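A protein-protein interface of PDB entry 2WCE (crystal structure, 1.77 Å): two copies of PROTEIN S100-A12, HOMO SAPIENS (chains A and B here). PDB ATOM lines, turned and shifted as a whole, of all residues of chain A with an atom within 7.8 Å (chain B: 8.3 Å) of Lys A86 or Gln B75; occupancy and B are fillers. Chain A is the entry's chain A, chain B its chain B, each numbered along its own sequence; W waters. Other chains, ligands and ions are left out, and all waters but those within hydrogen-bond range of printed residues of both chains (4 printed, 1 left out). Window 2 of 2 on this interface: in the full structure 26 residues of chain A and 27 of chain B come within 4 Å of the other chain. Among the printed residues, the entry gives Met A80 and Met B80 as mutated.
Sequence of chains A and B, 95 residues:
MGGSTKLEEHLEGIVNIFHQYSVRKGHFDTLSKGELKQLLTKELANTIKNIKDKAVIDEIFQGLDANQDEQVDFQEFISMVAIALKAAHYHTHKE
The side-chain amide oxygen of Gln B75 lies close to the side-chain amino group of Lys A86, 3.4 Å away.
O of Leu A85 lies within hydrogen-bond range of N of Tyr A90, 2.7 Å away. The backbone carbonyl oxygen (O) of Val B15 lies within hydrogen-bond range of a ring nitrogen (ND1) of His B19 (2.7 Å). The side-chain carboxylate of Asp B73 lies close to the backbone NH of Gln B75.
Ile A78 touches Ile B78. CG2 of Ile A78 touches CB of Ala B82 (3.8 Å). CD1 of Leu A85 touches CE2 of Phe B74 (3.998 Å). Tyr A90 touches Val B15 (CD1 to CG2, 3.9 Å). OH of Tyr A90 touches CB of Phe B74 (3.8 Å).
Of the printed residues of chain B, Ile A78 touches Ile B78 and Ala B82. Of the printed residues of chain B, Leu A85 touches Phe B74 (3.998 Å). Of chain B, only Gln B75 (3.4 Å) comes within 4 Å of Lys A86. No residue of chain B comes within 4 Å of Ala A87. Phe B18 touches none of the printed residues of chain A. Of the printed residues of chain A, Phe B74 touches Leu A85 (3.998 Å) and Tyr A90 (3.8 Å). Gln B75 touches just one residue of chain A: Lys A86 (3.4 Å). Of the printed residues of chain A, Ile B78 touches Ile A78 (3.8 Å). Printed residues of chain A within 4 Å of Ala B82: Ile A78. The nearest printed residue of chain B that does not touch Tyr A90 is His B19 (4.4 Å).
Along chain A the printed residues that touch a printed residue of chain B span positions 78 to 90. Of the 15 printed residues of chain B, 5 touch a printed residue of chain A. Among the printed residues, no Asp or Glu carboxylate lies within 4 Å of a Lys or Arg side-chain nitrogen of the other chain.
Ile B78 touches its own counterpart, Ile A78. Ile A78 touches Ala B82, but with the chains exchanged Ala A82 does not touch Ile B78 (4.3 Å). Positions printed for both chains: 78, 79, 80, 81 and 82. Of the 6 pairs that touch across the chains among the printed residues, 1 has its exchanged pair printed and touching as well.
Water W3 lies within hydrogen-bond range of the side-chain carboxylate (OD2) of Asp B73 (2.7 Å) and the side-chain amino group (NZ) of Lys A86 (2.8 Å). Water W1 bridges OH of Tyr A90 (2.8 Å) and NE2 of His B19 (2.9 Å). Water W4 lies within hydrogen-bond range of the side-chain hydroxyl of Tyr A90 (3.0 Å) and the backbone NH of Gln B75 (3.3 Å). Water W2 lies within hydrogen-bond range of the backbone carbonyl oxygen (O) of Ser A79 (3.0 Å) and the side-chain amide nitrogen (NE2) of Gln B75 (3.3 Å).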
ATOM      1  N   THR A  47      -9.815  -6.194  20.471  1.00  0.00           N
ATOM      2  CA  THR A  47      -9.680  -7.506  21.113  1.00  0.00           C
ATOM      3  C   THR A  47      -8.227  -7.720  21.599  1.00  0.00           C
ATOM      4  O   THR A  47      -7.997  -8.099  22.740  1.00  0.00           O
ATOM      5  CB  THR A  47     -10.098  -8.628  20.129  1.00  0.00           C
ATOM      6  OG1 THR A  47     -11.388  -8.346  19.622  1.00  0.00           O
ATOM      7  CG2 THR A  47     -10.098  -9.966  20.780  1.00  0.00           C
ATOM      8  N   ILE A  51      -6.457  -8.159  25.572  1.00  0.00           N
ATOM      9  CA  ILE A  51      -5.751  -9.322  26.117  1.00  0.00           C
ATOM     10  C   ILE A  51      -4.711  -8.855  27.143  1.00  0.00           C
ATOM     11  O   ILE A  51      -3.745  -8.144  26.817  1.00  0.00           O
ATOM     12  CB  ILE A  51      -5.060 -10.200  25.028  1.00  0.00           C
ATOM     13  CG1 ILE A  51      -6.055 -10.754  24.011  1.00  0.00           C
ATOM     14  CG2 ILE A  51      -4.355 -11.373  25.657  1.00  0.00           C
ATOM     15  CD1 ILE A  51      -5.382 -11.336  22.751  1.00  0.00           C
ATOM     16  N   VAL A  56       0.391 -14.231  24.668  1.00  0.00           N
ATOM     17  CA  VAL A  56      -0.554 -14.985  23.866  1.00  0.00           C
ATOM     18  C   VAL A  56      -0.455 -14.578  22.394  1.00  0.00           C
ATOM     19  O   VAL A  56      -0.351 -15.445  21.530  1.00  0.00           O
ATOM     20  CB  VAL A  56      -1.999 -14.797  24.390  1.00  0.00           C
ATOM     21  CG1 VAL A  56      -3.007 -15.482  23.485  1.00  0.00           C
ATOM     22  CG2 VAL A  56      -2.100 -15.317  25.843  1.00  0.00           C
ATOM     23  N   ILE A  78     -10.296 -18.748  11.332  1.00  0.00           N
ATOM     24  CA  ILE A  78     -11.341 -18.565  12.368  1.00  0.00           C
ATOM     25  C   ILE A  78     -10.893 -19.246  13.663  1.00  0.00           C
ATOM     26  O   ILE A  78     -11.208 -18.780  14.759  1.00  0.00           O
ATOM     27  CB  ILE A  78     -12.783 -18.907  11.791  1.00  0.00           C
ATOM     28  CG1 ILE A  78     -13.907 -18.216  12.605  1.00  0.00           C
ATOM     29  CG2 ILE A  78     -12.956 -20.320  11.734  1.00  0.00           C
ATOM     30  CD1 ILE A  78     -13.906 -16.718  12.560  1.00  0.00           C
ATOM     31  N   SER A  79     -10.152 -20.347  13.531  1.00  0.00           N
ATOM     32  CA  SER A  79      -9.476 -21.002  14.662  1.00  0.00           C
ATOM     33  C   SER A  79      -8.585 -20.032  15.438  1.00  0.00           C
ATOM     34  O   SER A  79      -8.694 -19.884  16.662  1.00  0.00           O
ATOM     35  CB  SER A  79      -8.617 -22.184  14.184  1.00  0.00           C
ATOM     36  OG  SER A  79      -7.735 -22.607  15.214  1.00  0.00           O
ATOM     37  N   MET A  80      -7.711 -19.355  14.707  1.00  0.00           N
ATOM     38  CA  MET A  80      -6.811 -18.399  15.312  1.00  0.00           C
ATOM     39  C   MET A  80      -7.552 -17.247  15.989  1.00  0.00           C
ATOM     40  O   MET A  80      -7.168 -16.834  17.104  1.00  0.00           O
ATOM     41  CB  MET A  80      -5.953 -17.843  14.226  1.00  0.00           C
ATOM     42  CG  MET A  80      -4.942 -16.953  14.645  1.00  0.00           C
ATOM     43  SD  MET A  80      -3.424 -17.662  13.646  1.00  0.00           S
ATOM     44  CE  MET A  80      -3.349 -19.201  14.965  1.00  0.00           C
ATOM     45  N   VAL A  81      -8.569 -16.722  15.304  1.00  0.00           N
ATOM     46  CA  VAL A  81      -9.447 -15.680  15.850  1.00  0.00           C
ATOM     47  C   VAL A  81     -10.049 -16.164  17.194  1.00  0.00           C
ATOM     48  O   VAL A  81     -10.050 -15.417  18.180  1.00  0.00           O
ATOM     49  CB  VAL A  81     -10.553 -15.285  14.868  1.00  0.00           C
ATOM     50  CG1 VAL A  81     -11.641 -14.491  15.550  1.00  0.00           C
ATOM     51  CG2 VAL A  81      -9.983 -14.513  13.654  1.00  0.00           C
ATOM     52  N   ALA A  82     -10.500 -17.426  17.246  1.00  0.00           N
ATOM     53  CA  ALA A  82     -11.108 -17.999  18.441  1.00  0.00           C
ATOM     54  C   ALA A  82     -10.113 -18.028  19.605  1.00  0.00           C
ATOM     55  O   ALA A  82     -10.479 -17.694  20.742  1.00  0.00           O
ATOM     56  CB  ALA A  82     -11.658 -19.409  18.157  1.00  0.00           C
ATOM     57  N   ILE A  83      -8.851 -18.367  19.332  1.00  0.00           N
ATOM     58  CA  ILE A  83      -7.782 -18.290  20.341  1.00  0.00           C
ATOM     59  C   ILE A  83      -7.654 -16.907  20.940  1.00  0.00           C
ATOM     60  O   ILE A  83      -7.630 -16.753  22.188  1.00  0.00           O
ATOM     61  CB  ILE A  83      -6.394 -18.782  19.794  1.00  0.00           C
ATOM     62  CG1 ILE A  83      -6.493 -20.268  19.450  1.00  0.00           C
ATOM     63  CG2 ILE A  83      -5.302 -18.532  20.830  1.00  0.00           C
ATOM     64  CD1 ILE A  83      -5.343 -20.788  18.564  1.00  0.00           C
ATOM     65  N   ALA A  84      -7.579 -15.914  20.075  1.00  0.00           N
ATOM     66  CA  ALA A  84      -7.399 -14.504  20.488  1.00  0.00           C
ATOM     67  C   ALA A  84      -8.617 -14.066  21.312  1.00  0.00           C
ATOM     68  O   ALA A  84      -8.488 -13.418  22.349  1.00  0.00           O
ATOM     69  CB  ALA A  84      -7.235 -13.604  19.254  1.00  0.00           C
ATOM     70  N   LEU A  85      -9.802 -14.466  20.855  1.00  0.00           N
ATOM     71  CA  LEU A  85     -11.046 -14.138  21.562  1.00  0.00           C
ATOM     72  C   LEU A  85     -11.087 -14.646  22.973  1.00  0.00           C
ATOM     73  O   LEU A  85     -11.519 -13.924  23.900  1.00  0.00           O
ATOM     74  CB  LEU A  85     -12.251 -14.714  20.817  1.00  0.00           C
ATOM     75  CG  LEU A  85     -12.820 -13.893  19.717  1.00  0.00           C
ATOM     76  CD1 LEU A  85     -14.032 -14.657  19.046  1.00  0.00           C
ATOM     77  CD2 LEU A  85     -13.299 -12.584  20.296  1.00  0.00           C
ATOM     78  N   LYS A  86     -10.671 -15.908  23.150  1.00  0.00           N
ATOM     79  CA  LYS A  86     -10.652 -16.511  24.429  1.00  0.00           C
ATOM     80  C   LYS A  86      -9.670 -15.782  25.313  1.00  0.00           C
ATOM     81  O   LYS A  86      -9.973 -15.555  26.468  1.00  0.00           O
ATOM     82  CB  LYS A  86     -10.285 -18.001  24.357  1.00  0.00           C
ATOM     83  CG  LYS A  86     -10.226 -18.724  25.702  1.00  0.00           C
ATOM     84  CD  LYS A  86      -9.832 -20.188  25.492  1.00  0.00           C
ATOM     85  CE  LYS A  86      -9.833 -20.985  26.771  1.00  0.00           C
ATOM     86  NZ  LYS A  86      -9.287 -22.381  26.605  1.00  0.00           N
ATOM     87  N   ALA A  87      -8.498 -15.427  24.776  1.00  0.00           N
ATOM     88  CA  ALA A  87      -7.460 -14.739  25.575  1.00  0.00           C
ATOM     89  C   ALA A  87      -7.955 -13.375  26.073  1.00  0.00           C
ATOM     90  O   ALA A  87      -7.556 -12.900  27.171  1.00  0.00           O
ATOM     91  CB  ALA A  87      -6.169 -14.583  24.733  1.00  0.00           C
ATOM     92  N   ALA A  88      -8.823 -12.755  25.272  1.00  0.00           N
ATOM     93  CA  ALA A  88      -9.457 -11.476  25.607  1.00  0.00           C
ATOM     94  C   ALA A  88     -10.673 -11.612  26.520  1.00  0.00           C
ATOM     95  O   ALA A  88     -11.342 -10.607  26.763  1.00  0.00           O
ATOM     96  CB  ALA A  88      -9.878 -10.718  24.316  1.00  0.00           C
ATOM     97  N   HIS A  89     -10.957 -12.795  27.074  1.00  0.00           N
ATOM     98  CA  HIS A  89     -12.210 -13.016  27.808  1.00  0.00           C
ATOM     99  C   HIS A  89     -13.419 -12.672  26.937  1.00  0.00           C
ATOM    100  O   HIS A  89     -14.457 -12.254  27.451  1.00  0.00           O
ATOM    101  CB  HIS A  89     -12.314 -12.149  29.073  1.00  0.00           C
ATOM    102  CG  HIS A  89     -11.466 -12.588  30.220  1.00  0.00           C
ATOM    103  ND1 HIS A  89     -10.225 -12.047  30.481  1.00  0.00           N
ATOM    104  CD2 HIS A  89     -11.722 -13.447  31.234  1.00  0.00           C
ATOM    105  CE1 HIS A  89      -9.734 -12.584  31.581  1.00  0.00           C
ATOM    106  NE2 HIS A  89     -10.620 -13.440  32.056  1.00  0.00           N
ATOM    107  N   TYR A  90     -13.299 -12.853  25.628  1.00  0.00           N
ATOM    108  CA  TYR A  90     -14.386 -12.495  24.690  1.00  0.00           C
ATOM    109  C   TYR A  90     -14.752 -10.983  24.682  1.00  0.00           C
ATOM    110  O   TYR A  90     -15.889 -10.614  24.351  1.00  0.00           O
ATOM    111  CB  TYR A  90     -15.642 -13.355  24.948  1.00  0.00           C
ATOM    112  CG  TYR A  90     -15.310 -14.831  25.046  1.00  0.00           C
ATOM    113  CD1 TYR A  90     -15.046 -15.575  23.908  1.00  0.00           C
ATOM    114  CD2 TYR A  90     -15.226 -15.470  26.275  1.00  0.00           C
ATOM    115  CE1 TYR A  90     -14.711 -16.914  23.982  1.00  0.00           C
ATOM    116  CE2 TYR A  90     -14.889 -16.823  26.361  1.00  0.00           C
ATOM    117  CZ  TYR A  90     -14.660 -17.537  25.179  1.00  0.00           C
ATOM    118  OH  TYR A  90     -14.314 -18.863  25.236  1.00  0.00           O
ATOM    119  N   HIS A  91     -13.802 -10.134  25.007  1.00  0.00           N
ATOM    120  CA  HIS A  91     -14.012  -8.686  24.978  1.00  0.00           C
ATOM    121  C   HIS A  91     -13.551  -8.158  23.633  1.00  0.00           C
ATOM    122  O   HIS A  91     -12.351  -8.063  23.397  1.00  0.00           O
ATOM    123  CB  HIS A  91     -13.249  -8.004  26.076  1.00  0.00           C
ATOM    124  CG  HIS A  91     -13.761  -8.316  27.442  1.00  0.00           C
ATOM    125  ND1 HIS A  91     -12.930  -8.616  28.496  1.00  0.00           N
ATOM    126  CD2 HIS A  91     -15.023  -8.403  27.915  1.00  0.00           C
ATOM    127  CE1 HIS A  91     -13.662  -8.850  29.572  1.00  0.00           C
ATOM    128  NE2 HIS A  91     -14.935  -8.737  29.242  1.00  0.00           N
ATOM    129  N   VAL B  15     -20.320 -15.024  19.807  1.00  0.00           N
ATOM    130  CA  VAL B  15     -20.040 -15.367  21.197  1.00  0.00           C
ATOM    131  C   VAL B  15     -21.303 -15.404  22.038  1.00  0.00           C
ATOM    132  O   VAL B  15     -21.495 -16.278  22.909  1.00  0.00           O
ATOM    133  CB  VAL B  15     -19.027 -14.357  21.799  1.00  0.00           C
ATOM    134  CG1 VAL B  15     -19.075 -14.439  23.326  1.00  0.00           C
ATOM    135  CG2 VAL B  15     -17.637 -14.628  21.221  1.00  0.00           C
ATOM    136  N   PHE B  18     -23.488 -18.557  21.112  1.00  0.00           N
ATOM    137  CA  PHE B  18     -22.920 -19.761  21.705  1.00  0.00           C
ATOM    138  C   PHE B  18     -23.346 -19.857  23.180  1.00  0.00           C
ATOM    139  O   PHE B  18     -23.794 -20.903  23.659  1.00  0.00           O
ATOM    140  CB  PHE B  18     -21.383 -19.809  21.609  1.00  0.00           C
ATOM    141  CG  PHE B  18     -20.766 -20.970  22.353  1.00  0.00           C
ATOM    142  CD1 PHE B  18     -20.774 -22.248  21.802  1.00  0.00           C
ATOM    143  CD2 PHE B  18     -20.287 -20.813  23.638  1.00  0.00           C
ATOM    144  CE1 PHE B  18     -20.215 -23.314  22.501  1.00  0.00           C
ATOM    145  CE2 PHE B  18     -19.750 -21.871  24.326  1.00  0.00           C
ATOM    146  CZ  PHE B  18     -19.715 -23.120  23.774  1.00  0.00           C
ATOM    147  N   HIS B  19     -23.113 -18.796  23.928  1.00  0.00           N
ATOM    148  CA  HIS B  19     -23.400 -18.825  25.368  1.00  0.00           C
ATOM    149  C   HIS B  19     -24.873 -18.925  25.728  1.00  0.00           C
ATOM    150  O   HIS B  19     -25.229 -19.465  26.781  1.00  0.00           O
ATOM    151  CB  HIS B  19     -22.687 -17.647  26.071  1.00  0.00           C
ATOM    152  CG  HIS B  19     -21.199 -17.807  26.094  1.00  0.00           C
ATOM    153  ND1 HIS B  19     -20.370 -17.281  25.125  1.00  0.00           N
ATOM    154  CD2 HIS B  19     -20.392 -18.479  26.954  1.00  0.00           C
ATOM    155  CE1 HIS B  19     -19.113 -17.587  25.415  1.00  0.00           C
ATOM    156  NE2 HIS B  19     -19.100 -18.331  26.508  1.00  0.00           N
ATOM    157  N   ASP B  29     -20.216 -22.632  30.187  1.00  0.00           N
ATOM    158  CA  ASP B  29     -19.517 -22.274  28.976  1.00  0.00           C
ATOM    159  C   ASP B  29     -19.191 -23.455  28.072  1.00  0.00           C
ATOM    160  O   ASP B  29     -18.434 -23.284  27.149  1.00  0.00           O
ATOM    161  CB  ASP B  29     -18.215 -21.515  29.310  1.00  0.00           C
ATOM    162  CG  ASP B  29     -17.229 -22.320  30.124  1.00  0.00           C
ATOM    163  OD1 ASP B  29     -16.100 -21.809  30.258  1.00  0.00           O
ATOM    164  OD2 ASP B  29     -17.516 -23.408  30.643  1.00  0.00           O
ATOM    165  N   VAL B  72     -18.134 -29.749  24.736  1.00  0.00           N
ATOM    166  CA  VAL B  72     -17.371 -28.971  23.774  1.00  0.00           C
ATOM    167  C   VAL B  72     -17.423 -27.483  24.141  1.00  0.00           C
ATOM    168  O   VAL B  72     -18.433 -26.973  24.649  1.00  0.00           O
ATOM    169  CB  VAL B  72     -17.885 -29.151  22.351  1.00  0.00           C
ATOM    170  CG1 VAL B  72     -18.058 -30.641  21.978  1.00  0.00           C
ATOM    171  CG2 VAL B  72     -19.121 -28.444  22.169  1.00  0.00           C
ATOM    172  N   ASP B  73     -16.319 -26.800  23.914  1.00  0.00           N
ATOM    173  CA  ASP B  73     -16.210 -25.381  24.279  1.00  0.00           C
ATOM    174  C   ASP B  73     -16.391 -24.498  23.034  1.00  0.00           C
ATOM    175  O   ASP B  73     -16.613 -25.009  21.902  1.00  0.00           O
ATOM    176  CB  ASP B  73     -14.878 -25.084  24.997  1.00  0.00           C
ATOM    177  CG  ASP B  73     -13.665 -25.344  24.142  1.00  0.00           C
ATOM    178  OD1 ASP B  73     -13.803 -25.567  22.914  1.00  0.00           O
ATOM    179  OD2 ASP B  73     -12.550 -25.338  24.728  1.00  0.00           O
ATOM    180  N   PHE B  74     -16.300 -23.192  23.240  1.00  0.00           N
ATOM    181  CA  PHE B  74     -16.471 -22.254  22.149  1.00  0.00           C
ATOM    182  C   PHE B  74     -15.542 -22.550  20.964  1.00  0.00           C
ATOM    183  O   PHE B  74     -15.986 -22.493  19.801  1.00  0.00           O
ATOM    184  CB  PHE B  74     -16.211 -20.853  22.628  1.00  0.00           C
ATOM    185  CG  PHE B  74     -16.347 -19.824  21.561  1.00  0.00           C
ATOM    186  CD1 PHE B  74     -17.601 -19.411  21.140  1.00  0.00           C
ATOM    187  CD2 PHE B  74     -15.231 -19.240  20.995  1.00  0.00           C
ATOM    188  CE1 PHE B  74     -17.756 -18.511  20.189  1.00  0.00           C
ATOM    189  CE2 PHE B  74     -15.385 -18.296  20.000  1.00  0.00           C
ATOM    190  CZ  PHE B  74     -16.632 -17.906  19.598  1.00  0.00           C
ATOM    191  N   GLN B  75     -14.278 -22.856  21.263  1.00  0.00           N
ATOM    192  CA  GLN B  75     -13.264 -23.139  20.196  1.00  0.00           C
ATOM    193  C   GLN B  75     -13.694 -24.293  19.302  1.00  0.00           C
ATOM    194  O   GLN B  75     -13.551 -24.251  18.065  1.00  0.00           O
ATOM    195  CB  GLN B  75     -11.909 -23.476  20.772  1.00  0.00           C
ATOM    196  CG  GLN B  75     -11.280 -22.329  21.415  1.00  0.00           C
ATOM    197  CD  GLN B  75      -9.987 -22.682  22.065  1.00  0.00           C
ATOM    198  OE1 GLN B  75      -9.908 -22.736  23.289  1.00  0.00           O
ATOM    199  NE2 GLN B  75      -8.958 -22.951  21.252  1.00  0.00           N
ATOM    200  N   GLU B  76     -14.244 -25.317  19.930  1.00  0.00           N
ATOM    201  CA  GLU B  76     -14.675 -26.477  19.186  1.00  0.00           C
ATOM    202  C   GLU B  76     -15.954 -26.219  18.384  1.00  0.00           C
ATOM    203  O   GLU B  76     -16.081 -26.721  17.250  1.00  0.00           O
ATOM    204  CB  GLU B  76     -14.783 -27.685  20.101  1.00  0.00           C
ATOM    205  CG  GLU B  76     -15.438 -28.888  19.453  1.00  0.00           C
ATOM    206  CD  GLU B  76     -14.885 -30.221  19.957  1.00  0.00           C
ATOM    207  OE1 GLU B  76     -14.484 -30.303  21.160  1.00  0.00           O
ATOM    208  OE2 GLU B  76     -14.849 -31.183  19.139  1.00  0.00           O
ATOM    209  N   PHE B  77     -16.880 -25.437  18.949  1.00  0.00           N
ATOM    210  CA  PHE B  77     -18.058 -25.005  18.281  1.00  0.00           C
ATOM    211  C   PHE B  77     -17.676 -24.258  16.996  1.00  0.00           C
ATOM    212  O   PHE B  77     -18.199 -24.556  15.909  1.00  0.00           O
ATOM    213  CB  PHE B  77     -18.887 -24.123  19.240  1.00  0.00           C
ATOM    214  CG  PHE B  77     -19.744 -23.133  18.584  1.00  0.00           C
ATOM    215  CD1 PHE B  77     -20.941 -23.486  18.017  1.00  0.00           C
ATOM    216  CD2 PHE B  77     -19.375 -21.789  18.561  1.00  0.00           C
ATOM    217  CE1 PHE B  77     -21.754 -22.523  17.449  1.00  0.00           C
ATOM    218  CE2 PHE B  77     -20.173 -20.820  17.980  1.00  0.00           C
ATOM    219  CZ  PHE B  77     -21.364 -21.179  17.403  1.00  0.00           C
ATOM    220  N   ILE B  78     -16.694 -23.373  17.123  1.00  0.00           N
ATOM    221  CA  ILE B  78     -16.242 -22.574  15.977  1.00  0.00           C
ATOM    222  C   ILE B  78     -15.706 -23.437  14.860  1.00  0.00           C
ATOM    223  O   ILE B  78     -16.001 -23.209  13.666  1.00  0.00           O
ATOM    224  CB  ILE B  78     -15.147 -21.553  16.429  1.00  0.00           C
ATOM    225  CG1 ILE B  78     -15.854 -20.391  17.058  1.00  0.00           C
ATOM    226  CG2 ILE B  78     -14.332 -21.126  15.237  1.00  0.00           C
ATOM    227  CD1 ILE B  78     -16.718 -19.571  16.060  1.00  0.00           C
ATOM    228  N   SER B  79     -14.922 -24.426  15.243  1.00  0.00           N
ATOM    229  CA  SER B  79     -14.345 -25.400  14.327  1.00  0.00           C
ATOM    230  C   SER B  79     -15.424 -26.159  13.564  1.00  0.00           C
ATOM    231  O   SER B  79     -15.317 -26.320  12.329  1.00  0.00           O
ATOM    232  CB  SER B  79     -13.472 -26.394  15.103  1.00  0.00           C
ATOM    233  OG  SER B  79     -13.258 -27.597  14.380  1.00  0.00           O
ATOM    234  N   MET B  80     -16.451 -26.614  14.276  1.00  0.00           N
ATOM    235  CA  MET B  80     -17.533 -27.336  13.630  1.00  0.00           C
ATOM    236  C   MET B  80     -18.309 -26.460  12.660  1.00  0.00           C
ATOM    237  O   MET B  80     -18.650 -26.904  11.545  1.00  0.00           O
ATOM    238  CB  MET B  80     -18.516 -27.926  14.655  1.00  0.00           C
ATOM    239  CG  MET B  80     -18.002 -29.088  15.469  1.00  0.00           C
ATOM    240  SD  MET B  80     -17.497 -30.631  14.393  1.00  0.00           S
ATOM    241  CE  MET B  80     -15.557 -30.161  14.295  1.00  0.00           C
ATOM    242  N   VAL B  81     -18.643 -25.244  13.091  1.00  0.00           N
ATOM    243  CA  VAL B  81     -19.318 -24.278  12.226  1.00  0.00           C
ATOM    244  C   VAL B  81     -18.493 -24.047  10.955  1.00  0.00           C
ATOM    245  O   VAL B  81     -19.054 -24.001   9.860  1.00  0.00           O
ATOM    246  CB  VAL B  81     -19.596 -22.969  12.992  1.00  0.00           C
ATOM    247  CG1 VAL B  81     -20.008 -21.847  12.061  1.00  0.00           C
ATOM    248  CG2 VAL B  81     -20.648 -23.225  14.113  1.00  0.00           C
ATOM    249  N   ALA B  82     -17.169 -23.868  11.102  1.00  0.00           N
ATOM    250  CA  ALA B  82     -16.292 -23.658   9.933  1.00  0.00           C
ATOM    251  C   ALA B  82     -16.334 -24.805   8.935  1.00  0.00           C
ATOM    252  O   ALA B  82     -16.299 -24.560   7.735  1.00  0.00           O
ATOM    253  CB  ALA B  82     -14.830 -23.356  10.365  1.00  0.00           C
HETATM  254  O   HOH W   1     -16.504 -19.620  26.828  1.00  0.00           O
HETATM  255  O   HOH W   2      -9.331 -22.453  18.061  1.00  0.00           O
HETATM  256  O   HOH W   3     -11.940 -23.164  26.126  1.00  0.00           O
HETATM  257  O   HOH W   4     -13.172 -21.308  23.944  1.00  0.00           O
